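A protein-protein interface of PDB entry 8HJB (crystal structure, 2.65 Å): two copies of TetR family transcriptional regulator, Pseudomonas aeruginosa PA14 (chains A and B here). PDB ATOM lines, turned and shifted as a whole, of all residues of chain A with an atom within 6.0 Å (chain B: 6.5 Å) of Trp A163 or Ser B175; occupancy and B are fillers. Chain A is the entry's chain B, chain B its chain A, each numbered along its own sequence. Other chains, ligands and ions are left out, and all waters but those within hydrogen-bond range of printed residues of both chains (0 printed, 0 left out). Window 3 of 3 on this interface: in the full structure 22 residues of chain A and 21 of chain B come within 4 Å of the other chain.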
ATOM      1  N   ARG A  96      -7.031 -11.343   9.810  1.00  0.00           N
ATOM      2  CA  ARG A  96      -7.959 -12.275  10.442  1.00  0.00           C
ATOM      3  C   ARG A  96      -8.545 -11.709  11.731  1.00  0.00           C
ATOM      4  O   ARG A  96      -9.750 -11.838  11.973  1.00  0.00           O
ATOM      5  CB  ARG A  96      -7.262 -13.608  10.716  1.00  0.00           C
ATOM      6  CG  ARG A  96      -6.495 -14.167   9.532  1.00  0.00           C
ATOM      7  CD  ARG A  96      -7.410 -14.442   8.352  1.00  0.00           C
ATOM      8  NE  ARG A  96      -8.265 -15.601   8.580  1.00  0.00           N
ATOM      9  CZ  ARG A  96      -9.433 -15.796   7.984  1.00  0.00           C
ATOM     10  NH1 ARG A  96      -9.919 -14.926   7.115  1.00  0.00           N
ATOM     11  NH2 ARG A  96     -10.130 -16.893   8.265  1.00  0.00           N
ATOM     12  N   TYR A 103     -15.980 -11.188  11.534  1.00  0.00           N
ATOM     13  CA  TYR A 103     -15.823 -12.636  11.622  1.00  0.00           C
ATOM     14  C   TYR A 103     -16.957 -13.251  12.432  1.00  0.00           C
ATOM     15  O   TYR A 103     -17.516 -14.286  12.048  1.00  0.00           O
ATOM     16  CB  TYR A 103     -14.460 -12.964  12.239  1.00  0.00           C
ATOM     17  CG  TYR A 103     -14.182 -14.433  12.511  1.00  0.00           C
ATOM     18  CD1 TYR A 103     -14.763 -15.088  13.592  1.00  0.00           C
ATOM     19  CD2 TYR A 103     -13.317 -15.155  11.700  1.00  0.00           C
ATOM     20  CE1 TYR A 103     -14.505 -16.421  13.845  1.00  0.00           C
ATOM     21  CE2 TYR A 103     -13.052 -16.490  11.949  1.00  0.00           C
ATOM     22  CZ  TYR A 103     -13.648 -17.117  13.022  1.00  0.00           C
ATOM     23  OH  TYR A 103     -13.389 -18.444  13.274  1.00  0.00           O
ATOM     24  N   HIS A 158      -0.007 -26.421  10.927  1.00  0.00           N
ATOM     25  CA  HIS A 158       0.250 -24.989  10.983  1.00  0.00           C
ATOM     26  C   HIS A 158      -1.010 -24.150  10.803  1.00  0.00           C
ATOM     27  O   HIS A 158      -1.226 -23.199  11.561  1.00  0.00           O
ATOM     28  CB  HIS A 158       1.280 -24.602   9.921  1.00  0.00           C
ATOM     29  CG  HIS A 158       2.683 -24.997  10.264  1.00  0.00           C
ATOM     30  ND1 HIS A 158       3.556 -24.152  10.916  1.00  0.00           N
ATOM     31  CD2 HIS A 158       3.366 -26.145  10.042  1.00  0.00           C
ATOM     32  CE1 HIS A 158       4.716 -24.764  11.083  1.00  0.00           C
ATOM     33  NE2 HIS A 158       4.627 -25.974  10.559  1.00  0.00           N
ATOM     34  N   TYR A 159      -1.849 -24.469   9.814  1.00  0.00           N
ATOM     35  CA  TYR A 159      -3.040 -23.661   9.582  1.00  0.00           C
ATOM     36  C   TYR A 159      -4.224 -24.080  10.442  1.00  0.00           C
ATOM     37  O   TYR A 159      -5.150 -23.282  10.623  1.00  0.00           O
ATOM     38  CB  TYR A 159      -3.427 -23.671   8.091  1.00  0.00           C
ATOM     39  CG  TYR A 159      -3.930 -24.981   7.507  1.00  0.00           C
ATOM     40  CD1 TYR A 159      -3.186 -25.666   6.555  1.00  0.00           C
ATOM     41  CD2 TYR A 159      -5.173 -25.500   7.857  1.00  0.00           C
ATOM     42  CE1 TYR A 159      -3.645 -26.846   6.001  1.00  0.00           C
ATOM     43  CE2 TYR A 159      -5.637 -26.681   7.311  1.00  0.00           C
ATOM     44  CZ  TYR A 159      -4.870 -27.350   6.383  1.00  0.00           C
ATOM     45  OH  TYR A 159      -5.334 -28.523   5.835  1.00  0.00           O
ATOM     46  N   CYS A 160      -4.225 -25.305  10.972  1.00  0.00           N
ATOM     47  CA  CYS A 160      -5.246 -25.666  11.949  1.00  0.00           C
ATOM     48  C   CYS A 160      -5.003 -24.952  13.272  1.00  0.00           C
ATOM     49  O   CYS A 160      -5.943 -24.432  13.885  1.00  0.00           O
ATOM     50  CB  CYS A 160      -5.279 -27.181  12.151  1.00  0.00           C
ATOM     51  SG  CYS A 160      -6.511 -28.043  11.147  1.00  0.00           S
ATOM     52  N   ALA A 161      -3.747 -24.909  13.720  1.00  0.00           N
ATOM     53  CA  ALA A 161      -3.408 -24.116  14.895  1.00  0.00           C
ATOM     54  C   ALA A 161      -3.578 -22.627  14.628  1.00  0.00           C
ATOM     55  O   ALA A 161      -3.950 -21.875  15.534  1.00  0.00           O
ATOM     56  CB  ALA A 161      -1.976 -24.417  15.337  1.00  0.00           C
ATOM     57  N   ALA A 162      -3.307 -22.185  13.398  1.00  0.00           N
ATOM     58  CA  ALA A 162      -3.556 -20.791  13.049  1.00  0.00           C
ATOM     59  C   ALA A 162      -5.047 -20.485  13.068  1.00  0.00           C
ATOM     60  O   ALA A 162      -5.458 -19.412  13.526  1.00  0.00           O
ATOM     61  CB  ALA A 162      -2.954 -20.473  11.680  1.00  0.00           C
ATOM     62  N   TRP A 163      -5.871 -21.415  12.579  1.00  0.00           N
ATOM     63  CA  TRP A 163      -7.317 -21.228  12.633  1.00  0.00           C
ATOM     64  C   TRP A 163      -7.817 -21.165  14.068  1.00  0.00           C
ATOM     65  O   TRP A 163      -8.770 -20.435  14.361  1.00  0.00           O
ATOM     66  CB  TRP A 163      -8.020 -22.358  11.877  1.00  0.00           C
ATOM     67  CG  TRP A 163      -9.516 -22.215  11.817  1.00  0.00           C
ATOM     68  CD1 TRP A 163     -10.247 -21.665  10.803  1.00  0.00           C
ATOM     69  CD2 TRP A 163     -10.462 -22.626  12.814  1.00  0.00           C
ATOM     70  NE1 TRP A 163     -11.587 -21.708  11.107  1.00  0.00           N
ATOM     71  CE2 TRP A 163     -11.745 -22.293  12.335  1.00  0.00           C
ATOM     72  CE3 TRP A 163     -10.349 -23.243  14.064  1.00  0.00           C
ATOM     73  CZ2 TRP A 163     -12.905 -22.556  13.061  1.00  0.00           C
ATOM     74  CZ3 TRP A 163     -11.500 -23.500  14.784  1.00  0.00           C
ATOM     75  CH2 TRP A 163     -12.762 -23.159  14.281  1.00  0.00           C
ATOM     76  N   ALA A 164      -7.189 -21.918  14.973  1.00  0.00           N
ATOM     77  CA  ALA A 164      -7.644 -21.942  16.359  1.00  0.00           C
ATOM     78  C   ALA A 164      -7.335 -20.630  17.068  1.00  0.00           C
ATOM     79  O   ALA A 164      -8.170 -20.116  17.820  1.00  0.00           O
ATOM     80  CB  ALA A 164      -7.006 -23.119  17.098  1.00  0.00           C
ATOM     81  N   LEU A 165      -6.143 -20.072  16.840  1.00  0.00           N
ATOM     82  CA  LEU A 165      -5.778 -18.821  17.496  1.00  0.00           C
ATOM     83  C   LEU A 165      -6.662 -17.672  17.028  1.00  0.00           C
ATOM     84  O   LEU A 165      -7.014 -16.788  17.818  1.00  0.00           O
ATOM     85  CB  LEU A 165      -4.305 -18.501  17.241  1.00  0.00           C
ATOM     86  CG  LEU A 165      -3.724 -17.368  18.089  1.00  0.00           C
ATOM     87  CD1 LEU A 165      -3.012 -17.918  19.315  1.00  0.00           C
ATOM     88  CD2 LEU A 165      -2.789 -16.495  17.263  1.00  0.00           C
ATOM     89  N   VAL A 166      -7.031 -17.668  15.747  1.00  0.00           N
ATOM     90  CA  VAL A 166      -7.932 -16.637  15.241  1.00  0.00           C
ATOM     91  C   VAL A 166      -9.325 -16.804  15.831  1.00  0.00           C
ATOM     92  O   VAL A 166     -10.003 -15.818  16.147  1.00  0.00           O
ATOM     93  CB  VAL A 166      -7.961 -16.660  13.702  1.00  0.00           C
ATOM     94  CG1 VAL A 166      -8.895 -15.587  13.176  1.00  0.00           C
ATOM     95  CG2 VAL A 166      -6.563 -16.443  13.148  1.00  0.00           C
ATOM     96  N   HIS A 167      -9.775 -18.049  15.998  1.00  0.00           N
ATOM     97  CA  HIS A 167     -11.127 -18.283  16.492  1.00  0.00           C
ATOM     98  C   HIS A 167     -11.259 -17.892  17.960  1.00  0.00           C
ATOM     99  O   HIS A 167     -12.149 -17.117  18.328  1.00  0.00           O
ATOM    100  CB  HIS A 167     -11.516 -19.747  16.292  1.00  0.00           C
ATOM    101  CG  HIS A 167     -12.989 -19.995  16.388  1.00  0.00           C
ATOM    102  ND1 HIS A 167     -13.880 -19.561  15.430  1.00  0.00           N
ATOM    103  CD2 HIS A 167     -13.729 -20.614  17.338  1.00  0.00           C
ATOM    104  CE1 HIS A 167     -15.105 -19.914  15.779  1.00  0.00           C
ATOM    105  NE2 HIS A 167     -15.041 -20.553  16.934  1.00  0.00           N
ATOM    106  N   GLY A 168     -10.383 -18.423  18.816  1.00  0.00           N
ATOM    107  CA  GLY A 168     -10.460 -18.131  20.236  1.00  0.00           C
ATOM    108  C   GLY A 168     -10.194 -16.683  20.586  1.00  0.00           C
ATOM    109  O   GLY A 168     -10.569 -16.240  21.677  1.00  0.00           O
ATOM    110  N   ARG B 104     -16.673 -28.485  25.906  1.00  0.00           N
ATOM    111  CA  ARG B 104     -17.882 -28.008  25.245  1.00  0.00           C
ATOM    112  C   ARG B 104     -19.133 -28.342  26.046  1.00  0.00           C
ATOM    113  O   ARG B 104     -20.131 -27.617  25.962  1.00  0.00           O
ATOM    114  CB  ARG B 104     -17.976 -28.592  23.836  1.00  0.00           C
ATOM    115  CG  ARG B 104     -18.699 -27.692  22.849  1.00  0.00           C
ATOM    116  CD  ARG B 104     -17.993 -26.351  22.712  1.00  0.00           C
ATOM    117  NE  ARG B 104     -17.230 -26.257  21.473  1.00  0.00           N
ATOM    118  CZ  ARG B 104     -17.728 -25.837  20.318  1.00  0.00           C
ATOM    119  NH1 ARG B 104     -18.991 -25.457  20.208  1.00  0.00           N
ATOM    120  NH2 ARG B 104     -16.941 -25.796  19.248  1.00  0.00           N
ATOM    121  N   GLY B 168     -10.065 -21.914  21.071  1.00  0.00           N
ATOM    122  CA  GLY B 168     -10.085 -22.127  19.634  1.00  0.00           C
ATOM    123  C   GLY B 168      -9.743 -23.548  19.240  1.00  0.00           C
ATOM    124  O   GLY B 168     -10.182 -24.025  18.189  1.00  0.00           O
ATOM    125  N   ALA B 169      -8.955 -24.239  20.068  1.00  0.00           N
ATOM    126  CA  ALA B 169      -8.633 -25.637  19.811  1.00  0.00           C
ATOM    127  C   ALA B 169      -9.826 -26.555  20.043  1.00  0.00           C
ATOM    128  O   ALA B 169     -10.002 -27.532  19.306  1.00  0.00           O
ATOM    129  CB  ALA B 169      -7.459 -26.080  20.685  1.00  0.00           C
ATOM    130  N   VAL B 170     -10.651 -26.273  21.056  1.00  0.00           N
ATOM    131  CA  VAL B 170     -11.860 -27.067  21.254  1.00  0.00           C
ATOM    132  C   VAL B 170     -12.807 -26.882  20.077  1.00  0.00           C
ATOM    133  O   VAL B 170     -13.398 -27.847  19.576  1.00  0.00           O
ATOM    134  CB  VAL B 170     -12.536 -26.707  22.590  1.00  0.00           C
ATOM    135  CG1 VAL B 170     -13.874 -27.418  22.707  1.00  0.00           C
ATOM    136  CG2 VAL B 170     -11.637 -27.083  23.756  1.00  0.00           C
ATOM    137  N   ALA B 171     -12.959 -25.640  19.609  1.00  0.00           N
ATOM    138  CA  ALA B 171     -13.757 -25.395  18.413  1.00  0.00           C
ATOM    139  C   ALA B 171     -13.117 -26.015  17.179  1.00  0.00           C
ATOM    140  O   ALA B 171     -13.828 -26.436  16.259  1.00  0.00           O
ATOM    141  CB  ALA B 171     -13.959 -23.895  18.214  1.00  0.00           C
ATOM    142  N   LEU B 172     -11.784 -26.077  17.140  1.00  0.00           N
ATOM    143  CA  LEU B 172     -11.101 -26.754  16.043  1.00  0.00           C
ATOM    144  C   LEU B 172     -11.394 -28.247  16.061  1.00  0.00           C
ATOM    145  O   LEU B 172     -11.749 -28.837  15.034  1.00  0.00           O
ATOM    146  CB  LEU B 172      -9.595 -26.499  16.125  1.00  0.00           C
ATOM    147  CG  LEU B 172      -8.712 -27.315  15.180  1.00  0.00           C
ATOM    148  CD1 LEU B 172      -9.064 -27.051  13.721  1.00  0.00           C
ATOM    149  CD2 LEU B 172      -7.239 -27.035  15.442  1.00  0.00           C
ATOM    150  N   TYR B 173     -11.253 -28.877  17.229  1.00  0.00           N
ATOM    151  CA  TYR B 173     -11.511 -30.306  17.346  1.00  0.00           C
ATOM    152  C   TYR B 173     -12.978 -30.648  17.122  1.00  0.00           C
ATOM    153  O   TYR B 173     -13.298 -31.813  16.859  1.00  0.00           O
ATOM    154  CB  TYR B 173     -11.062 -30.806  18.721  1.00  0.00           C
ATOM    155  CG  TYR B 173      -9.595 -31.172  18.799  1.00  0.00           C
ATOM    156  CD1 TYR B 173      -8.608 -30.214  18.610  1.00  0.00           C
ATOM    157  CD2 TYR B 173      -9.200 -32.476  19.064  1.00  0.00           C
ATOM    158  CE1 TYR B 173      -7.267 -30.543  18.682  1.00  0.00           C
ATOM    159  CE2 TYR B 173      -7.861 -32.814  19.138  1.00  0.00           C
ATOM    160  CZ  TYR B 173      -6.900 -31.844  18.946  1.00  0.00           C
ATOM    161  OH  TYR B 173      -5.566 -32.176  19.018  1.00  0.00           O
ATOM    162  N   HIS B 174     -13.874 -29.665  17.213  1.00  0.00           N
ATOM    163  CA  HIS B 174     -15.297 -29.891  16.995  1.00  0.00           C
ATOM    164  C   HIS B 174     -15.749 -29.548  15.581  1.00  0.00           C
ATOM    165  O   HIS B 174     -16.884 -29.878  15.217  1.00  0.00           O
ATOM    166  CB  HIS B 174     -16.123 -29.088  18.006  1.00  0.00           C
ATOM    167  CG  HIS B 174     -16.519 -29.877  19.215  1.00  0.00           C
ATOM    168  ND1 HIS B 174     -15.608 -30.299  20.158  1.00  0.00           N
ATOM    169  CD2 HIS B 174     -17.727 -30.326  19.630  1.00  0.00           C
ATOM    170  CE1 HIS B 174     -16.237 -30.973  21.105  1.00  0.00           C
ATOM    171  NE2 HIS B 174     -17.525 -31.002  20.808  1.00  0.00           N
ATOM    172  N   SER B 175     -14.905 -28.897  14.786  1.00  0.00           N
ATOM    173  CA  SER B 175     -15.212 -28.684  13.385  1.00  0.00           C
ATOM    174  C   SER B 175     -15.205 -30.021  12.648  1.00  0.00           C
ATOM    175  O   SER B 175     -14.662 -31.009  13.147  1.00  0.00           O
ATOM    176  CB  SER B 175     -14.194 -27.734  12.757  1.00  0.00           C
ATOM    177  OG  SER B 175     -14.263 -26.445  13.338  1.00  0.00           O
ATOM    178  N   PRO B 176     -15.815 -30.085  11.458  1.00  0.00           N
ATOM    179  CA  PRO B 176     -15.660 -31.288  10.626  1.00  0.00           C
ATOM    180  C   PRO B 176     -14.201 -31.570  10.293  1.00  0.00           C
ATOM    181  O   PRO B 176     -13.806 -31.581   9.123  1.00  0.00           O
ATOM    182  CB  PRO B 176     -16.473 -30.952   9.371  1.00  0.00           C
ATOM    183  CG  PRO B 176     -17.503 -29.990   9.842  1.00  0.00           C
ATOM    184  CD  PRO B 176     -16.860 -29.183  10.940  1.00  0.00           C
ATOM    185  N   PHE B 177     -13.395 -31.811  11.337  1.00  0.00           N
ATOM    186  CA  PHE B 177     -11.951 -31.964  11.180  1.00  0.00           C
ATOM    187  C   PHE B 177     -11.387 -32.985  12.164  1.00  0.00           C
ATOM    188  O   PHE B 177     -10.172 -32.991  12.395  1.00  0.00           O
ATOM    189  CB  PHE B 177     -11.244 -30.612  11.379  1.00  0.00           C
ATOM    190  CG  PHE B 177     -10.622 -30.061  10.128  1.00  0.00           C
ATOM    191  CD1 PHE B 177      -9.314 -30.371   9.796  1.00  0.00           C
ATOM    192  CD2 PHE B 177     -11.341 -29.226   9.288  1.00  0.00           C
ATOM    193  CE1 PHE B 177      -8.735 -29.864   8.646  1.00  0.00           C
ATOM    194  CE2 PHE B 177     -10.769 -28.717   8.138  1.00  0.00           C
ATOM    195  CZ  PHE B 177      -9.465 -29.036   7.816  1.00  0.00           C
ATOM    196  N   TRP B 178     -12.236 -33.826  12.758  1.00  0.00           N
ATOM    197  CA  TRP B 178     -11.778 -34.788  13.757  1.00  0.00           C
ATOM    198  C   TRP B 178     -10.761 -35.755  13.163  1.00  0.00           C
ATOM    199  O   TRP B 178      -9.674 -35.949  13.719  1.00  0.00           O
ATOM    200  CB  TRP B 178     -12.983 -35.539  14.328  1.00  0.00           C
ATOM    201  CG  TRP B 178     -12.664 -36.783  15.109  1.00  0.00           C
ATOM    202  CD1 TRP B 178     -11.589 -36.996  15.924  1.00  0.00           C
ATOM    203  CD2 TRP B 178     -13.436 -37.990  15.139  1.00  0.00           C
ATOM    204  NE1 TRP B 178     -11.646 -38.261  16.460  1.00  0.00           N
ATOM    205  CE2 TRP B 178     -12.769 -38.891  15.993  1.00  0.00           C
ATOM    206  CE3 TRP B 178     -14.625 -38.395  14.526  1.00  0.00           C
ATOM    207  CZ2 TRP B 178     -13.254 -40.172  16.249  1.00  0.00           C
ATOM    208  CZ3 TRP B 178     -15.104 -39.666  14.781  1.00  0.00           C
ATOM    209  CH2 TRP B 178     -14.420 -40.539  15.635  1.00  0.00           C
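The backbone carbonyl oxygen of Ala B171 sits at hydrogen-bond distance from the side-chain hydroxyl of Ser B175 (3.0 Å). A ring nitrogen (ND1) of His A167 lies within hydrogen-bond range of the side-chain hydroxyl of Tyr A103, at 2.5 Å.
Among the printed residues, pairs that only touch across the chains: Cys A160 with Leu B172, Ala A164 with Gly B168, His A167 with Ala B171, Trp A163 with Leu B172, Trp A163 with Gly B168, Ala A164 with Ala B169, Trp A163 with Ser B175, Gly A168 with Gly B168, Cys A160 with Phe B177 and Trp A163 with Ala B171.
Of the printed residues of chain B, Trp A163 touches Gly B168 (3.7 Å), Ala B171 (3.8 Å), Leu B172 (3.5 Å) and Ser B175 (3.7 Å). Of chain A, only Trp A163 (3.7 Å) comes within 4 Å of Ser B175. Printed residues of chain B within 4 Å of Cys A160: Leu B172 (3.3 Å) and Phe B177 (3.8 Å). Of the printed residues of chain A, Gly B168 touches Trp A163, Ala A164 and Gly A168. Of the printed residues of chain B, Gly A168 touches Gly B168. Printed residues of chain B within 4 Å of Ala A164: Gly B168 (3.3 Å) and Ala B169 (3.7 Å). Tyr B173 touches none of the printed residues of chain A. Tyr A159 touches none of the printed residues of chain B. The nearest printed residue of chain B that does not touch Trp A163 is Ala B169 (5.9 Å). The nearest printed residue of chain A that does not touch Ser B175 is His A167 (6.9 Å).
Of the 13 printed residues of chain A, 5 touch a printed residue of chain B. Printed residues of chain A that touch a printed residue of chain B: Cys A160, Trp A163, Ala A164, His A167 and Gly A168. Of the 12 printed residues of chain B, 6 touch a printed residue of chain A.
Gly A168 touches its own counterpart, Gly B168.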
